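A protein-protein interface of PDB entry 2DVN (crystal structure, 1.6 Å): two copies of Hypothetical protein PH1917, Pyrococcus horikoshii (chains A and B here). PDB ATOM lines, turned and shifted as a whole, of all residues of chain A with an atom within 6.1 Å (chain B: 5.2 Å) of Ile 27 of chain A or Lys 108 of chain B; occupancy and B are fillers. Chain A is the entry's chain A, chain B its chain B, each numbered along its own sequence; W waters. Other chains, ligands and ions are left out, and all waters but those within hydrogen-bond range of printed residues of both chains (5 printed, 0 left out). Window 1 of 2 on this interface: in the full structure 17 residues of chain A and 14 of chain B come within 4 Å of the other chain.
NZ of Lys 2 of chain A sits at hydrogen-bond distance from OH of Tyr 106 of chain B, 2.8 Å away.
The side-chain carboxylate (OE1) of Glu 26 of chain A is in salt-bridge range of the side-chain amino group (NZ) of Lys 108 of chain B (2.8 Å).
NZ of Lys 108 of chain B sits at hydrogen-bond distance from O of Ile 27 of chain A (3.3 Å).
The side-chain hydroxyl (OG) of Ser 123 of chain B sits at hydrogen-bond distance from the side-chain amide nitrogen (NE2) of Gln 29 of chain A, at 3.1 Å.
The backbone carbonyl oxygen of Glu 26 of chain A is in hydrogen-bond range of the backbone NH of Ile 3 of chain A (2.9 Å).
O of Ile 3 of chain A sits at hydrogen-bond distance from N of Val 28 of chain A, 3.0 Å away.
The backbone carbonyl oxygen (O) of Phe 4 of chain A is in hydrogen-bond range of the backbone NH (N) of Met 62 of chain A, at 2.8 Å.
The side-chain carboxylate of Glu 43 of chain B lies within salt-bridge range of the side-chain amino group of Lys 108 of chain B (2.7 Å).
O of Gly 67 of chain B is in hydrogen-bond range of N of Lys 108 of chain B, 3.0 Å away.
N of Phe 69 of chain B sits at hydrogen-bond distance from O of Tyr 106 of chain B (2.8 Å).
Tyr 106 of chain B touches Phe 4 of chain A (CE2 to CE2, 3.9 Å).
OE1 of Glu 26 of chain A touches OE1 of Glu 43 of chain B, 3.9 Å away.
Tyr 106 of chain B touches Val 28 of chain A (OH to CG2, 3.6 Å).
Val 125 of chain B touches Gln 29 of chain A.
Of the printed residues of chain B, Ile 27 of chain A touches Lys 108 (3.3 Å).
Of the printed residues of chain A, Lys 108 of chain B touches Glu 26 and Ile 27.
Printed residues of chain B within 4 Å of Val 28 of chain A: Tyr 106.
Printed residues of chain B within 4 Å of Phe 4 of chain A: Tyr 106.
Phe 107 of chain B touches none of the printed residues of chain A.
Val 110 of chain B touches none of the printed residues of chain A.
The nearest printed residue of chain B that does not touch Gln 29 of chain A is Gly 124 of chain B (4.1 Å).
Of the 16 printed residues of chain A, 6 touch a printed residue of chain B.
Hydrophobic or aromatic side chains of chain A within 4 Å of the printed part of chain B: Phe 4 and Val 28.
No position is printed for both chains.
Water W2 lies within hydrogen-bond range of the side-chain amide oxygen of Gln 29 of chain A, the backbone carbonyl oxygen of Ile 27 of chain A, the side-chain amino group of Lys 108 of chain B and the side-chain hydroxyl of Ser 123 of chain B.
Water W5 bridges OH of Tyr 106 of chain B (2.7 Å) and OE1 of Glu 26 of chain A (2.7 Å).
Water W1 lies within hydrogen-bond range of the side-chain carboxylate of Glu 26 of chain A, the side-chain carboxylate of Glu 43 of chain B and the backbone NH of Leu 42 of chain B.
Water W4 lies within hydrogen-bond range of OE2 of Glu 43 of chain B (2.9 Å) and N of Ile 27 of chain A (2.9 Å).
Water W3 bridges the backbone NH of Val 125 of chain B and the side-chain amide nitrogen of Gln 29 of chain A.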
ATOM      1  N   MET A   1      26.340   2.696  -2.622  1.00  0.00           N
ATOM      2  CA  MET A   1      25.111   1.922  -2.293  1.00  0.00           C
ATOM      3  C   MET A   1      23.876   2.484  -2.988  1.00  0.00           C
ATOM      4  O   MET A   1      23.685   3.698  -3.053  1.00  0.00           O
ATOM      5  CB  MET A   1      24.877   1.918  -0.780  1.00  0.00           C
ATOM      6  CG  MET A   1      23.561   1.278  -0.364  1.00  0.00           C
ATOM      7  SD  MET A   1      23.358   1.222   1.424  1.00  0.00           S
ATOM      8  CE  MET A   1      22.675   2.804   1.730  1.00  0.00           C
ATOM      9  N   LYS A   2      23.046   1.581  -3.494  1.00  0.00           N
ATOM     10  CA  LYS A   2      21.814   1.934  -4.184  1.00  0.00           C
ATOM     11  C   LYS A   2      20.671   1.196  -3.485  1.00  0.00           C
ATOM     12  O   LYS A   2      20.748  -0.011  -3.260  1.00  0.00           O
ATOM     13  CB  LYS A   2      21.911   1.523  -5.661  1.00  0.00           C
ATOM     14  CG  LYS A   2      20.655   1.764  -6.491  1.00  0.00           C
ATOM     15  CD  LYS A   2      20.910   1.579  -7.995  1.00  0.00           C
ATOM     16  CE  LYS A   2      21.752   0.348  -8.292  1.00  0.00           C
ATOM     17  NZ  LYS A   2      21.790  -0.004  -9.748  1.00  0.00           N
ATOM     18  N   ILE A   3      19.625   1.929  -3.123  1.00  0.00           N
ATOM     19  CA  ILE A   3      18.474   1.341  -2.449  1.00  0.00           C
ATOM     20  C   ILE A   3      17.229   1.496  -3.312  1.00  0.00           C
ATOM     21  O   ILE A   3      16.969   2.576  -3.843  1.00  0.00           O
ATOM     22  CB  ILE A   3      18.190   2.033  -1.102  1.00  0.00           C
ATOM     23  CG1 ILE A   3      19.411   1.930  -0.187  1.00  0.00           C
ATOM     24  CG2 ILE A   3      16.967   1.391  -0.438  1.00  0.00           C
ATOM     25  CD1 ILE A   3      19.241   2.660   1.129  1.00  0.00           C
ATOM     26  N   PHE A   4      16.459   0.420  -3.445  1.00  0.00           N
ATOM     27  CA  PHE A   4      15.238   0.467  -4.233  1.00  0.00           C
ATOM     28  C   PHE A   4      14.096   0.845  -3.307  1.00  0.00           C
ATOM     29  O   PHE A   4      13.832   0.167  -2.317  1.00  0.00           O
ATOM     30  CB  PHE A   4      14.993  -0.884  -4.900  1.00  0.00           C
ATOM     31  CG  PHE A   4      16.116  -1.305  -5.795  1.00  0.00           C
ATOM     32  CD1 PHE A   4      17.069  -2.226  -5.364  1.00  0.00           C
ATOM     33  CD2 PHE A   4      16.268  -0.716  -7.047  1.00  0.00           C
ATOM     34  CE1 PHE A   4      18.160  -2.551  -6.167  1.00  0.00           C
ATOM     35  CE2 PHE A   4      17.353  -1.033  -7.854  1.00  0.00           C
ATOM     36  CZ  PHE A   4      18.301  -1.952  -7.413  1.00  0.00           C
ATOM     37  N   PHE A   5      13.439   1.953  -3.627  1.00  0.00           N
ATOM     38  CA  PHE A   5      12.341   2.462  -2.814  1.00  0.00           C
ATOM     39  C   PHE A   5      11.025   2.095  -3.490  1.00  0.00           C
ATOM     40  O   PHE A   5      10.673   2.661  -4.527  1.00  0.00           O
ATOM     41  CB  PHE A   5      12.506   3.990  -2.678  1.00  0.00           C
ATOM     42  CG  PHE A   5      11.528   4.655  -1.736  1.00  0.00           C
ATOM     43  CD1 PHE A   5      10.668   3.911  -0.932  1.00  0.00           C
ATOM     44  CD2 PHE A   5      11.481   6.048  -1.653  1.00  0.00           C
ATOM     45  CE1 PHE A   5       9.774   4.544  -0.063  1.00  0.00           C
ATOM     46  CE2 PHE A   5      10.595   6.692  -0.787  1.00  0.00           C
ATOM     47  CZ  PHE A   5       9.739   5.936   0.009  1.00  0.00           C
ATOM     48  N   VAL A  13       9.575  10.128  -2.576  1.00  0.00           N
ATOM     49  CA  VAL A  13      10.801   9.864  -3.314  1.00  0.00           C
ATOM     50  C   VAL A  13      11.766  11.043  -3.242  1.00  0.00           C
ATOM     51  O   VAL A  13      12.941  10.865  -2.925  1.00  0.00           O
ATOM     52  CB  VAL A  13      10.510   9.539  -4.800  1.00  0.00           C
ATOM     53  CG1 VAL A  13      11.822   9.423  -5.575  1.00  0.00           C
ATOM     54  CG2 VAL A  13       9.731   8.236  -4.902  1.00  0.00           C
ATOM     55  N   VAL A  16      13.222  11.434   0.397  1.00  0.00           N
ATOM     56  CA  VAL A  16      14.164  10.378   0.735  1.00  0.00           C
ATOM     57  C   VAL A  16      15.460  10.528  -0.073  1.00  0.00           C
ATOM     58  O   VAL A  16      16.554  10.408   0.475  1.00  0.00           O
ATOM     59  CB  VAL A  16      13.536   8.987   0.475  1.00  0.00           C
ATOM     60  CG1 VAL A  16      14.591   7.890   0.614  1.00  0.00           C
ATOM     61  CG2 VAL A  16      12.401   8.749   1.462  1.00  0.00           C
ATOM     62  N   ALA A  17      15.334  10.806  -1.370  1.00  0.00           N
ATOM     63  CA  ALA A  17      16.503  10.965  -2.235  1.00  0.00           C
ATOM     64  C   ALA A  17      17.338  12.178  -1.843  1.00  0.00           C
ATOM     65  O   ALA A  17      18.568  12.132  -1.887  1.00  0.00           O
ATOM     66  CB  ALA A  17      16.064  11.081  -3.695  1.00  0.00           C
ATOM     67  N   LEU A  20      19.171  11.151   1.723  1.00  0.00           N
ATOM     68  CA  LEU A  20      20.233  10.165   1.585  1.00  0.00           C
ATOM     69  C   LEU A  20      21.273  10.514   0.527  1.00  0.00           C
ATOM     70  O   LEU A  20      22.418  10.055   0.602  1.00  0.00           O
ATOM     71  CB  LEU A  20      19.626   8.782   1.317  1.00  0.00           C
ATOM     72  CG  LEU A  20      18.762   8.258   2.474  1.00  0.00           C
ATOM     73  CD1 LEU A  20      18.064   6.973   2.060  1.00  0.00           C
ATOM     74  CD2 LEU A  20      19.632   8.031   3.709  1.00  0.00           C
ATOM     75  N   GLY A  21      20.885  11.335  -0.446  1.00  0.00           N
ATOM     76  CA  GLY A  21      21.816  11.730  -1.490  1.00  0.00           C
ATOM     77  C   GLY A  21      22.970  12.533  -0.920  1.00  0.00           C
ATOM     78  O   GLY A  21      24.067  12.556  -1.478  1.00  0.00           O
ATOM     79  N   ILE A  25      24.254   8.126  -1.220  1.00  0.00           N
ATOM     80  CA  ILE A  25      23.408   6.956  -1.413  1.00  0.00           C
ATOM     81  C   ILE A  25      22.388   7.239  -2.514  1.00  0.00           C
ATOM     82  O   ILE A  25      21.707   8.266  -2.489  1.00  0.00           O
ATOM     83  CB  ILE A  25      22.677   6.598  -0.103  1.00  0.00           C
ATOM     84  CG1 ILE A  25      23.705   6.195   0.957  1.00  0.00           C
ATOM     85  CG2 ILE A  25      21.682   5.467  -0.340  1.00  0.00           C
ATOM     86  CD1 ILE A  25      23.128   6.048   2.352  1.00  0.00           C
ATOM     87  N   GLU A  26      22.299   6.335  -3.485  1.00  0.00           N
ATOM     88  CA  GLU A  26      21.366   6.491  -4.595  1.00  0.00           C
ATOM     89  C   GLU A  26      20.034   5.809  -4.299  1.00  0.00           C
ATOM     90  O   GLU A  26      19.993   4.718  -3.731  1.00  0.00           O
ATOM     91  CB  GLU A  26      21.952   5.897  -5.887  1.00  0.00           C
ATOM     92  CG  GLU A  26      21.016   6.036  -7.088  1.00  0.00           C
ATOM     93  CD  GLU A  26      21.510   5.348  -8.349  1.00  0.00           C
ATOM     94  OE1 GLU A  26      20.793   5.437  -9.368  1.00  0.00           O
ATOM     95  OE2 GLU A  26      22.593   4.719  -8.331  1.00  0.00           O
ATOM     96  N   ILE A  27      18.945   6.463  -4.685  1.00  0.00           N
ATOM     97  CA  ILE A  27      17.617   5.913  -4.501  1.00  0.00           C
ATOM     98  C   ILE A  27      17.044   5.639  -5.886  1.00  0.00           C
ATOM     99  O   ILE A  27      17.137   6.487  -6.776  1.00  0.00           O
ATOM    100  CB  ILE A  27      16.689   6.915  -3.776  1.00  0.00           C
ATOM    101  CG1 ILE A  27      17.191   7.158  -2.351  1.00  0.00           C
ATOM    102  CG2 ILE A  27      15.253   6.401  -3.783  1.00  0.00           C
ATOM    103  CD1 ILE A  27      17.165   5.935  -1.461  1.00  0.00           C
ATOM    104  N   VAL A  28      16.491   4.447  -6.076  1.00  0.00           N
ATOM    105  CA  VAL A  28      15.869   4.099  -7.347  1.00  0.00           C
ATOM    106  C   VAL A  28      14.436   3.691  -7.028  1.00  0.00           C
ATOM    107  O   VAL A  28      14.187   2.634  -6.442  1.00  0.00           O
ATOM    108  CB  VAL A  28      16.591   2.930  -8.060  1.00  0.00           C
ATOM    109  CG1 VAL A  28      15.836   2.564  -9.344  1.00  0.00           C
ATOM    110  CG2 VAL A  28      18.029   3.322  -8.392  1.00  0.00           C
ATOM    111  N   GLN A  29      13.495   4.547  -7.405  1.00  0.00           N
ATOM    112  CA  GLN A  29      12.089   4.287  -7.152  1.00  0.00           C
ATOM    113  C   GLN A  29      11.574   3.120  -7.991  1.00  0.00           C
ATOM    114  O   GLN A  29      11.996   2.912  -9.131  1.00  0.00           O
ATOM    115  CB  GLN A  29      11.259   5.543  -7.438  1.00  0.00           C
ATOM    116  CG  GLN A  29      11.414   6.083  -8.850  1.00  0.00           C
ATOM    117  CD  GLN A  29      12.467   7.178  -8.969  1.00  0.00           C
ATOM    118  OE1 GLN A  29      13.598   7.038  -8.493  1.00  0.00           O
ATOM    119  NE2 GLN A  29      12.096   8.276  -9.623  1.00  0.00           N
ATOM    120  N   MET A  62      13.384  -0.593   0.340  1.00  0.00           N
ATOM    121  CA  MET A  62      12.743   0.078   1.454  1.00  0.00           C
ATOM    122  C   MET A  62      11.325   0.462   1.058  1.00  0.00           C
ATOM    123  O   MET A  62      11.013   0.617  -0.129  1.00  0.00           O
ATOM    124  CB  MET A  62      13.521   1.342   1.843  1.00  0.00           C
ATOM    125  CG  MET A  62      13.516   2.433   0.779  1.00  0.00           C
ATOM    126  SD  MET A  62      14.412   3.929   1.286  1.00  0.00           S
ATOM    127  CE  MET A  62      13.254   4.703   2.316  1.00  0.00           C
ATOM    128  N   LEU B  42      24.008   8.522 -12.371  1.00  0.00           N
ATOM    129  CA  LEU B  42      23.658   9.566 -13.329  1.00  0.00           C
ATOM    130  C   LEU B  42      23.650  10.895 -12.578  1.00  0.00           C
ATOM    131  O   LEU B  42      23.968  11.945 -13.138  1.00  0.00           O
ATOM    132  CB  LEU B  42      22.271   9.316 -13.933  1.00  0.00           C
ATOM    133  CG  LEU B  42      22.111   8.103 -14.851  1.00  0.00           C
ATOM    134  CD1 LEU B  42      20.630   7.786 -15.007  1.00  0.00           C
ATOM    135  CD2 LEU B  42      22.750   8.392 -16.202  1.00  0.00           C
ATOM    136  N   GLU B  43      23.286  10.843 -11.300  1.00  0.00           N
ATOM    137  CA  GLU B  43      23.247  12.049 -10.483  1.00  0.00           C
ATOM    138  C   GLU B  43      24.601  12.754 -10.419  1.00  0.00           C
ATOM    139  O   GLU B  43      24.665  13.985 -10.407  1.00  0.00           O
ATOM    140  CB  GLU B  43      22.767  11.722  -9.064  1.00  0.00           C
ATOM    141  CG  GLU B  43      21.273  11.457  -8.967  1.00  0.00           C
ATOM    142  CD  GLU B  43      20.903   9.998  -9.163  1.00  0.00           C
ATOM    143  OE1 GLU B  43      21.699   9.233  -9.748  1.00  0.00           O
ATOM    144  OE2 GLU B  43      19.796   9.615  -8.733  1.00  0.00           O
ATOM    145  N   ASP B  65      20.578  13.163 -18.511  1.00  0.00           N
ATOM    146  CA  ASP B  65      21.374  11.980 -18.800  1.00  0.00           C
ATOM    147  C   ASP B  65      20.539  10.784 -18.373  1.00  0.00           C
ATOM    148  O   ASP B  65      19.775  10.861 -17.413  1.00  0.00           O
ATOM    149  CB  ASP B  65      22.704  12.008 -18.039  1.00  0.00           C
ATOM    150  CG  ASP B  65      23.702  10.976 -18.559  1.00  0.00           C
ATOM    151  OD1 ASP B  65      23.531  10.495 -19.700  1.00  0.00           O
ATOM    152  OD2 ASP B  65      24.670  10.654 -17.833  1.00  0.00           O
ATOM    153  N   SER B  66      20.662   9.683 -19.101  1.00  0.00           N
ATOM    154  CA  SER B  66      19.898   8.493 -18.772  1.00  0.00           C
ATOM    155  C   SER B  66      20.683   7.260 -19.156  1.00  0.00           C
ATOM    156  O   SER B  66      21.734   7.356 -19.792  1.00  0.00           O
ATOM    157  CB  SER B  66      18.564   8.490 -19.515  1.00  0.00           C
ATOM    158  OG  SER B  66      18.779   8.381 -20.908  1.00  0.00           O
ATOM    159  N   GLY B  67      20.163   6.102 -18.769  1.00  0.00           N
ATOM    160  CA  GLY B  67      20.834   4.860 -19.097  1.00  0.00           C
ATOM    161  C   GLY B  67      20.010   3.646 -18.728  1.00  0.00           C
ATOM    162  O   GLY B  67      18.981   3.758 -18.054  1.00  0.00           O
ATOM    163  N   PHE B  69      20.031   0.054 -16.789  1.00  0.00           N
ATOM    164  CA  PHE B  69      20.734  -0.627 -15.705  1.00  0.00           C
ATOM    165  C   PHE B  69      20.206  -2.051 -15.580  1.00  0.00           C
ATOM    166  O   PHE B  69      19.060  -2.265 -15.179  1.00  0.00           O
ATOM    167  CB  PHE B  69      20.514   0.150 -14.399  1.00  0.00           C
ATOM    168  CG  PHE B  69      21.064   1.552 -14.430  1.00  0.00           C
ATOM    169  CD1 PHE B  69      22.294   1.843 -13.846  1.00  0.00           C
ATOM    170  CD2 PHE B  69      20.371   2.573 -15.079  1.00  0.00           C
ATOM    171  CE1 PHE B  69      22.830   3.129 -13.909  1.00  0.00           C
ATOM    172  CE2 PHE B  69      20.901   3.866 -15.148  1.00  0.00           C
ATOM    173  CZ  PHE B  69      22.134   4.140 -14.561  1.00  0.00           C
ATOM    174  N   TYR B 106      16.150  -1.682 -15.589  1.00  0.00           N
ATOM    175  CA  TYR B 106      15.384  -0.451 -15.562  1.00  0.00           C
ATOM    176  C   TYR B 106      16.104   0.666 -16.291  1.00  0.00           C
ATOM    177  O   TYR B 106      17.338   0.692 -16.371  1.00  0.00           O
ATOM    178  CB  TYR B 106      15.082  -0.013 -14.115  1.00  0.00           C
ATOM    179  CG  TYR B 106      16.292   0.373 -13.279  1.00  0.00           C
ATOM    180  CD1 TYR B 106      16.858   1.650 -13.362  1.00  0.00           C
ATOM    181  CD2 TYR B 106      16.871  -0.543 -12.407  1.00  0.00           C
ATOM    182  CE1 TYR B 106      17.977   1.998 -12.591  1.00  0.00           C
ATOM    183  CE2 TYR B 106      17.982  -0.210 -11.636  1.00  0.00           C
ATOM    184  CZ  TYR B 106      18.532   1.056 -11.731  1.00  0.00           C
ATOM    185  OH  TYR B 106      19.644   1.363 -10.971  1.00  0.00           O
ATOM    186  N   PHE B 107      15.310   1.566 -16.858  1.00  0.00           N
ATOM    187  CA  PHE B 107      15.836   2.744 -17.527  1.00  0.00           C
ATOM    188  C   PHE B 107      15.663   3.845 -16.492  1.00  0.00           C
ATOM    189  O   PHE B 107      14.635   3.901 -15.814  1.00  0.00           O
ATOM    190  CB  PHE B 107      14.994   3.113 -18.754  1.00  0.00           C
ATOM    191  CG  PHE B 107      15.439   2.461 -20.033  1.00  0.00           C
ATOM    192  CD1 PHE B 107      16.666   2.780 -20.601  1.00  0.00           C
ATOM    193  CD2 PHE B 107      14.610   1.560 -20.692  1.00  0.00           C
ATOM    194  CE1 PHE B 107      17.060   2.210 -21.809  1.00  0.00           C
ATOM    195  CE2 PHE B 107      14.999   0.987 -21.903  1.00  0.00           C
ATOM    196  CZ  PHE B 107      16.225   1.316 -22.459  1.00  0.00           C
ATOM    197  N   LYS B 108      16.662   4.707 -16.349  1.00  0.00           N
ATOM    198  CA  LYS B 108      16.555   5.818 -15.413  1.00  0.00           C
ATOM    199  C   LYS B 108      17.018   7.087 -16.108  1.00  0.00           C
ATOM    200  O   LYS B 108      18.006   7.079 -16.843  1.00  0.00           O
ATOM    201  CB  LYS B 108      17.402   5.575 -14.152  1.00  0.00           C
ATOM    202  CG  LYS B 108      17.395   6.749 -13.166  1.00  0.00           C
ATOM    203  CD  LYS B 108      18.028   6.389 -11.822  1.00  0.00           C
ATOM    204  CE  LYS B 108      18.168   7.622 -10.938  1.00  0.00           C
ATOM    205  NZ  LYS B 108      18.684   7.278  -9.582  1.00  0.00           N
ATOM    206  N   SER B 109      16.279   8.168 -15.889  1.00  0.00           N
ATOM    207  CA  SER B 109      16.611   9.464 -16.461  1.00  0.00           C
ATOM    208  C   SER B 109      16.732  10.477 -15.334  1.00  0.00           C
ATOM    209  O   SER B 109      15.924  10.478 -14.403  1.00  0.00           O
ATOM    210  CB  SER B 109      15.516   9.924 -17.432  1.00  0.00           C
ATOM    211  OG  SER B 109      15.676  11.296 -17.763  1.00  0.00           O
ATOM    212  N   VAL B 110      17.759  11.318 -15.403  1.00  0.00           N
ATOM    213  CA  VAL B 110      17.954  12.359 -14.408  1.00  0.00           C
ATOM    214  C   VAL B 110      18.078  13.695 -15.122  1.00  0.00           C
ATOM    215  O   VAL B 110      18.887  13.856 -16.039  1.00  0.00           O
ATOM    216  CB  VAL B 110      19.227  12.131 -13.555  1.00  0.00           C
ATOM    217  CG1 VAL B 110      19.445  13.319 -12.616  1.00  0.00           C
ATOM    218  CG2 VAL B 110      19.087  10.856 -12.744  1.00  0.00           C
ATOM    219  N   SER B 123      14.164  12.804 -11.274  1.00  0.00           N
ATOM    220  CA  SER B 123      14.377  11.530 -11.939  1.00  0.00           C
ATOM    221  C   SER B 123      13.100  10.813 -12.336  1.00  0.00           C
ATOM    222  O   SER B 123      12.011  11.113 -11.837  1.00  0.00           O
ATOM    223  CB  SER B 123      15.208  10.609 -11.050  1.00  0.00           C
ATOM    224  OG  SER B 123      14.498  10.278  -9.871  1.00  0.00           O
ATOM    225  N   GLY B 124      13.263   9.866 -13.251  1.00  0.00           N
ATOM    226  CA  GLY B 124      12.168   9.051 -13.738  1.00  0.00           C
ATOM    227  C   GLY B 124      12.740   7.663 -13.956  1.00  0.00           C
ATOM    228  O   GLY B 124      13.851   7.529 -14.458  1.00  0.00           O
ATOM    229  N   VAL B 125      11.988   6.632 -13.583  1.00  0.00           N
ATOM    230  CA  VAL B 125      12.449   5.255 -13.720  1.00  0.00           C
ATOM    231  C   VAL B 125      11.372   4.357 -14.310  1.00  0.00           C
ATOM    232  O   VAL B 125      10.205   4.437 -13.922  1.00  0.00           O
ATOM    233  CB  VAL B 125      12.852   4.668 -12.341  1.00  0.00           C
ATOM    234  CG1 VAL B 125      13.315   3.228 -12.495  1.00  0.00           C
ATOM    235  CG2 VAL B 125      13.943   5.521 -11.710  1.00  0.00           C
ATOM    236  N   THR B 126      11.769   3.510 -15.255  1.00  0.00           N
ATOM    237  CA  THR B 126      10.848   2.568 -15.871  1.00  0.00           C
ATOM    238  C   THR B 126      11.468   1.181 -15.785  1.00  0.00           C
ATOM    239  O   THR B 126      12.548   0.934 -16.329  1.00  0.00           O
ATOM    240  CB  THR B 126      10.574   2.922 -17.342  1.00  0.00           C
ATOM    241  OG1 THR B 126       9.897   4.184 -17.403  1.00  0.00           O
ATOM    242  CG2 THR B 126       9.705   1.847 -18.002  1.00  0.00           C
ATOM    243  N   HIS B 168      10.777   6.673 -19.188  1.00  0.00           N
ATOM    244  CA  HIS B 168      11.443   7.104 -17.967  1.00  0.00           C
ATOM    245  C   HIS B 168      11.750   8.597 -18.064  1.00  0.00           C
ATOM    246  O   HIS B 168      11.704   9.316 -17.061  1.00  0.00           O
ATOM    247  CB  HIS B 168      12.744   6.318 -17.763  1.00  0.00           C
ATOM    248  CG  HIS B 168      13.592   6.229 -18.992  1.00  0.00           C
ATOM    249  ND1 HIS B 168      13.180   5.572 -20.133  1.00  0.00           N
ATOM    250  CD2 HIS B 168      14.826   6.716 -19.264  1.00  0.00           C
ATOM    251  CE1 HIS B 168      14.124   5.661 -21.053  1.00  0.00           C
ATOM    252  NE2 HIS B 168      15.133   6.349 -20.552  1.00  0.00           N
HETATM  253  O   HOH W   1      21.718   7.007 -11.484  1.00  0.00           O
HETATM  254  O   HOH W   2      15.999   7.907  -8.904  1.00  0.00           O
HETATM  255  O   HOH W   3       9.759   7.469 -11.761  1.00  0.00           O
HETATM  256  O   HOH W   4      19.218   9.123  -5.919  1.00  0.00           O
HETATM  257  O   HOH W   5      20.714   3.751 -11.448  1.00  0.00           O
